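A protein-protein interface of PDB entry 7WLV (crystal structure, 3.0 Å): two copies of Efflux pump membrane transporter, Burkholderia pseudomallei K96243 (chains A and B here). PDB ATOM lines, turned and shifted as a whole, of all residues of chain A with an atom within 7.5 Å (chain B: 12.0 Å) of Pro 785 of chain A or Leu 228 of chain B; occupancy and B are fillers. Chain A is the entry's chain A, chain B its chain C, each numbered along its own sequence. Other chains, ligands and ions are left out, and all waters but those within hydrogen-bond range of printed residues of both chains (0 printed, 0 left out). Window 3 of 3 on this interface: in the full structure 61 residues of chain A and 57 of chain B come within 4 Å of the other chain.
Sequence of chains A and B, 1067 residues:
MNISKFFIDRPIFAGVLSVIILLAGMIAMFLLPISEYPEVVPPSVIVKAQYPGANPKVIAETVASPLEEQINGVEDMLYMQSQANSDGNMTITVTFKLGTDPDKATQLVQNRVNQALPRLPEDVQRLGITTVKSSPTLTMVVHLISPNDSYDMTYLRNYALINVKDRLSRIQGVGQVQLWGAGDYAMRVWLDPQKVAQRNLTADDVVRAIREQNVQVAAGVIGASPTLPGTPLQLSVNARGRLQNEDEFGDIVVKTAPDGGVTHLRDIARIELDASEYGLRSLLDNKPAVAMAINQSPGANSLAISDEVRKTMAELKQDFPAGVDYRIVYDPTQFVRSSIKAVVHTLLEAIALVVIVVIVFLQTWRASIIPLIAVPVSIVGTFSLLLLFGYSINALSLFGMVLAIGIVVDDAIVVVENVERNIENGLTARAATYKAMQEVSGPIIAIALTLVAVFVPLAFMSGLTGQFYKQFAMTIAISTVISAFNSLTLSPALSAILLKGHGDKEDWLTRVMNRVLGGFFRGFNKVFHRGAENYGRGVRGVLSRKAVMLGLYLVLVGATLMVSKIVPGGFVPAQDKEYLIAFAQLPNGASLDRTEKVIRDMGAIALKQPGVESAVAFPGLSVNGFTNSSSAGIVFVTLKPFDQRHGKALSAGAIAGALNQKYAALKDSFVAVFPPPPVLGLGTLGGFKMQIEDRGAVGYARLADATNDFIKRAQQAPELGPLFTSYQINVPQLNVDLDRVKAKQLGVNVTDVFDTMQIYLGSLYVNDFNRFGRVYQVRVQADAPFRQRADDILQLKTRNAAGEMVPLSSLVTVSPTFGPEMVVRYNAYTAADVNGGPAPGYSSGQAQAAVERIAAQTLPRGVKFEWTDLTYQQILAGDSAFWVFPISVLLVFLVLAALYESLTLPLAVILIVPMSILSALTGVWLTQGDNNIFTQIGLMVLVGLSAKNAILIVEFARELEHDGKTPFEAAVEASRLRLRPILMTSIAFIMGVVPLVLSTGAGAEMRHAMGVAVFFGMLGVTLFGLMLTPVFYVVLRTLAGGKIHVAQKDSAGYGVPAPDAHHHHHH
O of Arg 787 of chain A is in hydrogen-bond range of N of Gly 223 of chain B, 2.8 Å away.
The guanidinium group (NH1) of Arg 787 of chain A sits at hydrogen-bond distance from the backbone carbonyl oxygen (O) of Ala 224 of chain B, 3.2 Å away.
The backbone carbonyl oxygen (O) of Pro 226 of chain B sits at hydrogen-bond distance from the guanidinium group (NH2) of Arg 787 of chain A, 3.3 Å away.
O of Ala 782 of chain A is in hydrogen-bond range of NE of Arg 787 of chain A (2.6 Å).
The backbone carbonyl oxygen (O) of Gly 223 of chain B is in hydrogen-bond range of the side-chain hydroxyl (OG1) of Thr 227 of chain B, at 3.2 Å.
OG1 of Thr 227 of chain B is in hydrogen-bond range of O of Ala 224 of chain B (2.9 Å).
Among the printed residues, merely in contact across the chains: Asp 593 of chain A with Thr 227 of chain B, Ala 784 of chain A with Pro 226 of chain B, Ala 784 of chain A with Thr 227 of chain B, Pro 785 of chain A with Leu 228 of chain B, Arg 787 of chain A with Ile 222 of chain B, Gln 788 of chain A with Ile 222 of chain B, Gln 788 of chain A with Gly 223 of chain B, Gln 788 of chain A with Thr 227 of chain B, Gln 788 of chain A with Leu 228 of chain B, Gln 788 of chain A with Pro 229 of chain B and Arg 789 of chain A with Ile 222 of chain B.
Of chain B, only Leu 228 comes within 4 Å of Pro 785 of chain A.
No residue of chain B comes within 4 Å of Asp 783 of chain A.
No residue of chain B comes within 4 Å of Phe 786 of chain A.
Of chain B, only Ile 222 (3.2 Å), Gly 223 (2.8 Å), Ala 224 (3.2 Å) and Pro 226 (3.3 Å) come within 4 Å of Arg 787 of chain A.
Of chain B, only Ile 222, Gly 223, Thr 227, Leu 228 and Pro 229 come within 4 Å of Gln 788 of chain A.
No residue of chain B comes within 4 Å of Asp 792 of chain A.
Printed residues of chain A within 4 Å of Pro 226 of chain B: Ala 784 (3.4 Å) and Arg 787 (3.3 Å).
Of the printed residues of chain B, Arg 789 of chain A touches Ile 222 (3.1 Å).
Of the printed residues of chain A, Thr 227 of chain B touches Asp 593, Ala 784 and Gln 788.
Gln 194 of chain A touches none of the printed residues of chain B.
The nearest residue of chain B that does not touch Pro 785 of chain A is Thr 227 of chain B (5.4 Å).
The nearest residue of chain A that does not touch Leu 228 of chain B is Ala 784 of chain A (4.3 Å).
The nearest printed residue of chain A that does not touch Pro 226 of chain B is Trp 190 of chain A (4.03 Å).
Among the printed residues, 14 pairs touch across the chains.
No position is printed for both chains.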
ATOM      1  N   TRP A 190     -22.252  -7.559   4.784  1.00  0.00           N
ATOM      2  CA  TRP A 190     -23.036  -8.777   4.628  1.00  0.00           C
ATOM      3  C   TRP A 190     -24.157  -8.707   5.642  1.00  0.00           C
ATOM      4  O   TRP A 190     -23.930  -8.951   6.825  1.00  0.00           O
ATOM      5  CB  TRP A 190     -22.155 -10.003   4.850  1.00  0.00           C
ATOM      6  CG  TRP A 190     -20.902 -10.066   3.950  1.00  0.00           C
ATOM      7  CD1 TRP A 190     -19.602  -9.859   4.331  1.00  0.00           C
ATOM      8  CD2 TRP A 190     -20.861 -10.374   2.545  1.00  0.00           C
ATOM      9  NE1 TRP A 190     -18.760 -10.012   3.254  1.00  0.00           N
ATOM     10  CE2 TRP A 190     -19.503 -10.336   2.148  1.00  0.00           C
ATOM     11  CE3 TRP A 190     -21.836 -10.690   1.589  1.00  0.00           C
ATOM     12  CZ2 TRP A 190     -19.095 -10.602   0.835  1.00  0.00           C
ATOM     13  CZ3 TRP A 190     -21.430 -10.951   0.283  1.00  0.00           C
ATOM     14  CH2 TRP A 190     -20.068 -10.901  -0.083  1.00  0.00           C
ATOM     15  N   LEU A 191     -25.350  -8.325   5.188  1.00  0.00           N
ATOM     16  CA  LEU A 191     -26.473  -8.133   6.097  1.00  0.00           C
ATOM     17  C   LEU A 191     -27.009  -9.456   6.636  1.00  0.00           C
ATOM     18  O   LEU A 191     -27.135 -10.440   5.908  1.00  0.00           O
ATOM     19  CB  LEU A 191     -27.606  -7.373   5.414  1.00  0.00           C
ATOM     20  CG  LEU A 191     -27.414  -5.906   5.019  1.00  0.00           C
ATOM     21  CD1 LEU A 191     -28.778  -5.312   4.692  1.00  0.00           C
ATOM     22  CD2 LEU A 191     -26.729  -5.092   6.104  1.00  0.00           C
ATOM     23  N   PRO A 193     -30.349 -10.554   7.579  1.00  0.00           N
ATOM     24  CA  PRO A 193     -31.723 -10.039   7.443  1.00  0.00           C
ATOM     25  C   PRO A 193     -32.626 -10.333   8.648  1.00  0.00           C
ATOM     26  O   PRO A 193     -33.490  -9.508   8.984  1.00  0.00           O
ATOM     27  CB  PRO A 193     -32.216 -10.716   6.157  1.00  0.00           C
ATOM     28  CG  PRO A 193     -31.335 -11.885   5.976  1.00  0.00           C
ATOM     29  CD  PRO A 193     -30.008 -11.527   6.536  1.00  0.00           C
ATOM     30  N   GLN A 194     -32.426 -11.460   9.339  1.00  0.00           N
ATOM     31  CA  GLN A 194     -33.117 -11.671  10.607  1.00  0.00           C
ATOM     32  C   GLN A 194     -32.817 -10.531  11.571  1.00  0.00           C
ATOM     33  O   GLN A 194     -33.735  -9.936  12.147  1.00  0.00           O
ATOM     34  CB  GLN A 194     -32.724 -13.023  11.213  1.00  0.00           C
ATOM     35  CG  GLN A 194     -33.157 -14.212  10.353  1.00  0.00           C
ATOM     36  CD  GLN A 194     -32.506 -15.546  10.730  1.00  0.00           C
ATOM     37  OE1 GLN A 194     -31.503 -15.587  11.445  1.00  0.00           O
ATOM     38  NE2 GLN A 194     -33.035 -16.639  10.179  1.00  0.00           N
ATOM     39  N   ARG A 270     -22.173  -8.069   8.970  1.00  0.00           N
ATOM     40  CA  ARG A 270     -20.760  -8.398   9.069  1.00  0.00           C
ATOM     41  C   ARG A 270     -20.021  -7.532   8.054  1.00  0.00           C
ATOM     42  O   ARG A 270     -20.418  -7.485   6.893  1.00  0.00           O
ATOM     43  CB  ARG A 270     -20.593  -9.894   8.800  1.00  0.00           C
ATOM     44  CG  ARG A 270     -19.245 -10.470   9.074  1.00  0.00           C
ATOM     45  CD  ARG A 270     -19.228 -11.975   8.839  1.00  0.00           C
ATOM     46  NE  ARG A 270     -18.225 -12.333   7.835  1.00  0.00           N
ATOM     47  CZ  ARG A 270     -18.502 -12.715   6.593  1.00  0.00           C
ATOM     48  NH1 ARG A 270     -19.748 -12.856   6.174  1.00  0.00           N
ATOM     49  NH2 ARG A 270     -17.502 -12.931   5.742  1.00  0.00           N
ATOM     50  N   ASP A 593     -17.919 -23.414  -6.479  1.00  0.00           N
ATOM     51  CA  ASP A 593     -17.007 -24.184  -5.630  1.00  0.00           C
ATOM     52  C   ASP A 593     -16.807 -25.613  -6.136  1.00  0.00           C
ATOM     53  O   ASP A 593     -15.675 -26.131  -6.123  1.00  0.00           O
ATOM     54  CB  ASP A 593     -17.514 -24.196  -4.199  1.00  0.00           C
ATOM     55  CG  ASP A 593     -17.357 -22.868  -3.531  1.00  0.00           C
ATOM     56  OD1 ASP A 593     -17.400 -21.825  -4.228  1.00  0.00           O
ATOM     57  OD2 ASP A 593     -17.186 -22.880  -2.296  1.00  0.00           O
ATOM     58  N   ALA A 782     -27.177  -9.556   1.525  1.00  0.00           N
ATOM     59  CA  ALA A 782     -27.383 -10.555   2.565  1.00  0.00           C
ATOM     60  C   ALA A 782     -26.181 -11.482   2.655  1.00  0.00           C
ATOM     61  O   ALA A 782     -25.545 -11.801   1.644  1.00  0.00           O
ATOM     62  CB  ALA A 782     -28.646 -11.369   2.315  1.00  0.00           C
ATOM     63  N   ASP A 783     -25.868 -11.906   3.877  1.00  0.00           N
ATOM     64  CA  ASP A 783     -24.759 -12.819   4.103  1.00  0.00           C
ATOM     65  C   ASP A 783     -25.048 -14.183   3.488  1.00  0.00           C
ATOM     66  O   ASP A 783     -26.199 -14.570   3.274  1.00  0.00           O
ATOM     67  CB  ASP A 783     -24.498 -12.999   5.592  1.00  0.00           C
ATOM     68  CG  ASP A 783     -23.084 -13.438   5.893  1.00  0.00           C
ATOM     69  OD1 ASP A 783     -22.552 -14.315   5.194  1.00  0.00           O
ATOM     70  OD2 ASP A 783     -22.499 -12.935   6.857  1.00  0.00           O
ATOM     71  N   ALA A 784     -23.968 -14.929   3.247  1.00  0.00           N
ATOM     72  CA  ALA A 784     -24.050 -16.240   2.609  1.00  0.00           C
ATOM     73  C   ALA A 784     -25.054 -17.185   3.264  1.00  0.00           C
ATOM     74  O   ALA A 784     -25.830 -17.818   2.528  1.00  0.00           O
ATOM     75  CB  ALA A 784     -22.643 -16.847   2.568  1.00  0.00           C
ATOM     76  N   PRO A 785     -25.095 -17.346   4.596  1.00  0.00           N
ATOM     77  CA  PRO A 785     -26.058 -18.293   5.180  1.00  0.00           C
ATOM     78  C   PRO A 785     -27.494 -17.906   4.939  1.00  0.00           C
ATOM     79  O   PRO A 785     -28.393 -18.720   5.168  1.00  0.00           O
ATOM     80  CB  PRO A 785     -25.706 -18.291   6.673  1.00  0.00           C
ATOM     81  CG  PRO A 785     -24.334 -17.793   6.735  1.00  0.00           C
ATOM     82  CD  PRO A 785     -24.230 -16.783   5.642  1.00  0.00           C
ATOM     83  N   PHE A 786     -27.749 -16.671   4.538  1.00  0.00           N
ATOM     84  CA  PHE A 786     -29.100 -16.176   4.368  1.00  0.00           C
ATOM     85  C   PHE A 786     -29.562 -16.125   2.912  1.00  0.00           C
ATOM     86  O   PHE A 786     -30.649 -15.599   2.646  1.00  0.00           O
ATOM     87  CB  PHE A 786     -29.191 -14.815   5.024  1.00  0.00           C
ATOM     88  CG  PHE A 786     -28.748 -14.832   6.455  1.00  0.00           C
ATOM     89  CD1 PHE A 786     -29.541 -15.432   7.422  1.00  0.00           C
ATOM     90  CD2 PHE A 786     -27.513 -14.315   6.828  1.00  0.00           C
ATOM     91  CE1 PHE A 786     -29.142 -15.462   8.736  1.00  0.00           C
ATOM     92  CE2 PHE A 786     -27.103 -14.352   8.146  1.00  0.00           C
ATOM     93  CZ  PHE A 786     -27.914 -14.928   9.097  1.00  0.00           C
ATOM     94  N   ARG A 787     -28.767 -16.639   1.957  1.00  0.00           N
ATOM     95  CA  ARG A 787     -29.173 -16.662   0.551  1.00  0.00           C
ATOM     96  C   ARG A 787     -28.917 -17.991  -0.169  1.00  0.00           C
ATOM     97  O   ARG A 787     -29.002 -18.030  -1.408  1.00  0.00           O
ATOM     98  CB  ARG A 787     -28.515 -15.510  -0.234  1.00  0.00           C
ATOM     99  CG  ARG A 787     -27.089 -15.166   0.154  1.00  0.00           C
ATOM    100  CD  ARG A 787     -26.551 -13.950  -0.634  1.00  0.00           C
ATOM    101  NE  ARG A 787     -25.195 -13.635  -0.201  1.00  0.00           N
ATOM    102  CZ  ARG A 787     -24.099 -14.234  -0.643  1.00  0.00           C
ATOM    103  NH1 ARG A 787     -24.139 -15.141  -1.610  1.00  0.00           N
ATOM    104  NH2 ARG A 787     -22.934 -13.947  -0.070  1.00  0.00           N
ATOM    105  N   GLN A 788     -28.601 -19.075   0.542  1.00  0.00           N
ATOM    106  CA  GLN A 788     -28.227 -20.331  -0.114  1.00  0.00           C
ATOM    107  C   GLN A 788     -29.399 -21.297  -0.226  1.00  0.00           C
ATOM    108  O   GLN A 788     -29.213 -22.515  -0.157  1.00  0.00           O
ATOM    109  CB  GLN A 788     -27.085 -20.990   0.646  1.00  0.00           C
ATOM    110  CG  GLN A 788     -27.420 -21.263   2.095  1.00  0.00           C
ATOM    111  CD  GLN A 788     -26.422 -22.181   2.771  1.00  0.00           C
ATOM    112  OE1 GLN A 788     -25.456 -21.724   3.386  1.00  0.00           O
ATOM    113  NE2 GLN A 788     -26.656 -23.486   2.670  1.00  0.00           N
ATOM    114  N   ARG A 789     -30.594 -20.787  -0.506  1.00  0.00           N
ATOM    115  CA  ARG A 789     -31.815 -21.542  -0.251  1.00  0.00           C
ATOM    116  C   ARG A 789     -33.017 -20.772  -0.768  1.00  0.00           C
ATOM    117  O   ARG A 789     -33.080 -19.554  -0.564  1.00  0.00           O
ATOM    118  CB  ARG A 789     -31.919 -21.802   1.259  1.00  0.00           C
ATOM    119  CG  ARG A 789     -33.016 -22.719   1.741  1.00  0.00           C
ATOM    120  CD  ARG A 789     -34.210 -21.864   2.068  1.00  0.00           C
ATOM    121  NE  ARG A 789     -35.372 -22.603   2.551  1.00  0.00           N
ATOM    122  CZ  ARG A 789     -36.154 -23.354   1.787  1.00  0.00           C
ATOM    123  NH1 ARG A 789     -35.865 -23.582   0.510  1.00  0.00           N
ATOM    124  NH2 ARG A 789     -37.245 -23.882   2.318  1.00  0.00           N
ATOM    125  N   ASP A 792     -35.008 -18.756   1.723  1.00  0.00           N
ATOM    126  CA  ASP A 792     -34.300 -17.622   2.279  1.00  0.00           C
ATOM    127  C   ASP A 792     -34.730 -16.356   1.541  1.00  0.00           C
ATOM    128  O   ASP A 792     -34.468 -15.236   2.006  1.00  0.00           O
ATOM    129  CB  ASP A 792     -32.787 -17.833   2.192  1.00  0.00           C
ATOM    130  CG  ASP A 792     -32.279 -18.826   3.235  1.00  0.00           C
ATOM    131  OD1 ASP A 792     -32.923 -18.956   4.287  1.00  0.00           O
ATOM    132  OD2 ASP A 792     -31.211 -19.437   3.031  1.00  0.00           O
ATOM    133  N   VAL B 221     -29.793 -13.843  -6.946  1.00  0.00           N
ATOM    134  CA  VAL B 221     -29.257 -15.170  -7.231  1.00  0.00           C
ATOM    135  C   VAL B 221     -29.108 -15.914  -5.913  1.00  0.00           C
ATOM    136  O   VAL B 221     -28.532 -15.387  -4.955  1.00  0.00           O
ATOM    137  CB  VAL B 221     -27.907 -15.108  -7.975  1.00  0.00           C
ATOM    138  CG1 VAL B 221     -27.339 -16.485  -8.148  1.00  0.00           C
ATOM    139  CG2 VAL B 221     -28.093 -14.468  -9.311  1.00  0.00           C
ATOM    140  N   ILE B 222     -29.605 -17.137  -5.869  1.00  0.00           N
ATOM    141  CA  ILE B 222     -29.527 -17.958  -4.673  1.00  0.00           C
ATOM    142  C   ILE B 222     -28.289 -18.834  -4.753  1.00  0.00           C
ATOM    143  O   ILE B 222     -28.030 -19.470  -5.780  1.00  0.00           O
ATOM    144  CB  ILE B 222     -30.799 -18.805  -4.510  1.00  0.00           C
ATOM    145  CG1 ILE B 222     -31.962 -17.918  -4.088  1.00  0.00           C
ATOM    146  CG2 ILE B 222     -30.573 -19.916  -3.516  1.00  0.00           C
ATOM    147  CD1 ILE B 222     -31.668 -17.097  -2.882  1.00  0.00           C
ATOM    148  N   GLY B 223     -27.510 -18.852  -3.677  1.00  0.00           N
ATOM    149  CA  GLY B 223     -26.389 -19.764  -3.614  1.00  0.00           C
ATOM    150  C   GLY B 223     -25.186 -19.355  -4.421  1.00  0.00           C
ATOM    151  O   GLY B 223     -24.346 -20.204  -4.717  1.00  0.00           O
ATOM    152  N   ALA B 224     -25.077 -18.074  -4.780  1.00  0.00           N
ATOM    153  CA  ALA B 224     -23.968 -17.536  -5.550  1.00  0.00           C
ATOM    154  C   ALA B 224     -22.733 -17.342  -4.671  1.00  0.00           C
ATOM    155  O   ALA B 224     -22.781 -17.402  -3.443  1.00  0.00           O
ATOM    156  CB  ALA B 224     -24.364 -16.218  -6.218  1.00  0.00           C
ATOM    157  N   SER B 225     -21.615 -17.098  -5.323  1.00  0.00           N
ATOM    158  CA  SER B 225     -20.375 -16.956  -4.590  1.00  0.00           C
ATOM    159  C   SER B 225     -20.324 -15.628  -3.835  1.00  0.00           C
ATOM    160  O   SER B 225     -20.800 -14.602  -4.331  1.00  0.00           O
ATOM    161  CB  SER B 225     -19.191 -17.064  -5.535  1.00  0.00           C
ATOM    162  OG  SER B 225     -18.044 -17.447  -4.805  1.00  0.00           O
ATOM    163  N   PRO B 226     -19.746 -15.622  -2.631  1.00  0.00           N
ATOM    164  CA  PRO B 226     -19.274 -16.819  -1.918  1.00  0.00           C
ATOM    165  C   PRO B 226     -20.380 -17.440  -1.056  1.00  0.00           C
ATOM    166  O   PRO B 226     -21.213 -16.703  -0.535  1.00  0.00           O
ATOM    167  CB  PRO B 226     -18.098 -16.279  -1.089  1.00  0.00           C
ATOM    168  CG  PRO B 226     -18.441 -14.837  -0.834  1.00  0.00           C
ATOM    169  CD  PRO B 226     -19.299 -14.372  -1.988  1.00  0.00           C
ATOM    170  N   THR B 227     -20.435 -18.772  -0.935  1.00  0.00           N
ATOM    171  CA  THR B 227     -21.349 -19.478  -0.037  1.00  0.00           C
ATOM    172  C   THR B 227     -20.554 -20.577   0.649  1.00  0.00           C
ATOM    173  O   THR B 227     -19.595 -21.115   0.082  1.00  0.00           O
ATOM    174  CB  THR B 227     -22.558 -20.104  -0.739  1.00  0.00           C
ATOM    175  OG1 THR B 227     -22.427 -19.959  -2.165  1.00  0.00           O
ATOM    176  CG2 THR B 227     -23.864 -19.477  -0.218  1.00  0.00           C
ATOM    177  N   LEU B 228     -20.941 -20.895   1.865  1.00  0.00           N
ATOM    178  CA  LEU B 228     -20.037 -21.713   2.666  1.00  0.00           C
ATOM    179  C   LEU B 228     -19.978 -23.229   2.465  1.00  0.00           C
ATOM    180  O   LEU B 228     -18.902 -23.781   2.231  1.00  0.00           O
ATOM    181  CB  LEU B 228     -20.306 -21.407   4.152  1.00  0.00           C
ATOM    182  CG  LEU B 228     -21.608 -21.643   4.938  1.00  0.00           C
ATOM    183  CD1 LEU B 228     -21.327 -21.614   6.439  1.00  0.00           C
ATOM    184  CD2 LEU B 228     -22.705 -20.664   4.568  1.00  0.00           C
ATOM    185  N   PRO B 229     -21.033 -23.945   2.683  1.00  0.00           N
ATOM    186  CA  PRO B 229     -20.824 -25.360   3.001  1.00  0.00           C
ATOM    187  C   PRO B 229     -20.518 -26.279   1.846  1.00  0.00           C
ATOM    188  O   PRO B 229     -19.382 -26.676   1.593  1.00  0.00           O
ATOM    189  CB  PRO B 229     -22.163 -25.758   3.651  1.00  0.00           C
ATOM    190  CG  PRO B 229     -23.200 -24.716   3.133  1.00  0.00           C
ATOM    191  CD  PRO B 229     -22.427 -23.688   2.292  1.00  0.00           C
ATOM    192  N   GLY B 230     -21.584 -26.576   1.133  1.00  0.00           N
ATOM    193  CA  GLY B 230     -21.603 -27.447  -0.005  1.00  0.00           C
ATOM    194  C   GLY B 230     -22.737 -27.042  -0.907  1.00  0.00           C
ATOM    195  O   GLY B 230     -23.329 -27.905  -1.561  1.00  0.00           O
ATOM    196  N   THR B 231     -23.105 -25.764  -0.889  1.00  0.00           N
ATOM    197  CA  THR B 231     -24.178 -25.283  -1.743  1.00  0.00           C
ATOM    198  C   THR B 231     -24.047 -25.863  -3.144  1.00  0.00           C
ATOM    199  O   THR B 231     -23.080 -25.577  -3.856  1.00  0.00           O
ATOM    200  CB  THR B 231     -24.141 -23.768  -1.791  1.00  0.00           C
ATOM    201  OG1 THR B 231     -23.912 -23.266  -0.463  1.00  0.00           O
ATOM    202  CG2 THR B 231     -25.447 -23.237  -2.357  1.00  0.00           C
ATOM    203  N   PRO B 232     -25.006 -26.693  -3.566  1.00  0.00           N
ATOM    204  CA  PRO B 232     -24.807 -27.530  -4.757  1.00  0.00           C
ATOM    205  C   PRO B 232     -25.024 -26.779  -6.055  1.00  0.00           C
ATOM    206  O   PRO B 232     -24.426 -27.092  -7.084  1.00  0.00           O
ATOM    207  CB  PRO B 232     -25.860 -28.630  -4.574  1.00  0.00           C
ATOM    208  CG  PRO B 232     -26.973 -27.925  -3.904  1.00  0.00           C
ATOM    209  CD  PRO B 232     -26.354 -26.870  -3.002  1.00  0.00           C
ATOM    210  N   LEU B 233     -25.940 -25.830  -6.013  1.00  0.00           N
ATOM    211  CA  LEU B 233     -26.424 -25.150  -7.190  1.00  0.00           C
ATOM    212  C   LEU B 233     -26.367 -23.657  -6.955  1.00  0.00           C
ATOM    213  O   LEU B 233     -26.374 -23.182  -5.819  1.00  0.00           O
ATOM    214  CB  LEU B 233     -27.857 -25.535  -7.534  1.00  0.00           C
ATOM    215  CG  LEU B 233     -28.115 -26.956  -8.026  1.00  0.00           C
ATOM    216  CD1 LEU B 233     -29.492 -27.026  -8.691  1.00  0.00           C
ATOM    217  CD2 LEU B 233     -27.006 -27.471  -8.934  1.00  0.00           C
ATOM    218  N   GLN B 234     -26.260 -22.930  -8.048  1.00  0.00           N
ATOM    219  CA  GLN B 234     -26.364 -21.483  -8.058  1.00  0.00           C
ATOM    220  C   GLN B 234     -27.576 -21.138  -8.911  1.00  0.00           C
ATOM    221  O   GLN B 234     -27.559 -21.333 -10.132  1.00  0.00           O
ATOM    222  CB  GLN B 234     -25.060 -20.896  -8.577  1.00  0.00           C
ATOM    223  CG  GLN B 234     -25.061 -19.460  -8.899  1.00  0.00           C
ATOM    224  CD  GLN B 234     -23.641 -18.988  -9.014  1.00  0.00           C
ATOM    225  OE1 GLN B 234     -22.759 -19.524  -8.320  1.00  0.00           O
ATOM    226  NE2 GLN B 234     -23.395 -17.988  -9.865  1.00  0.00           N
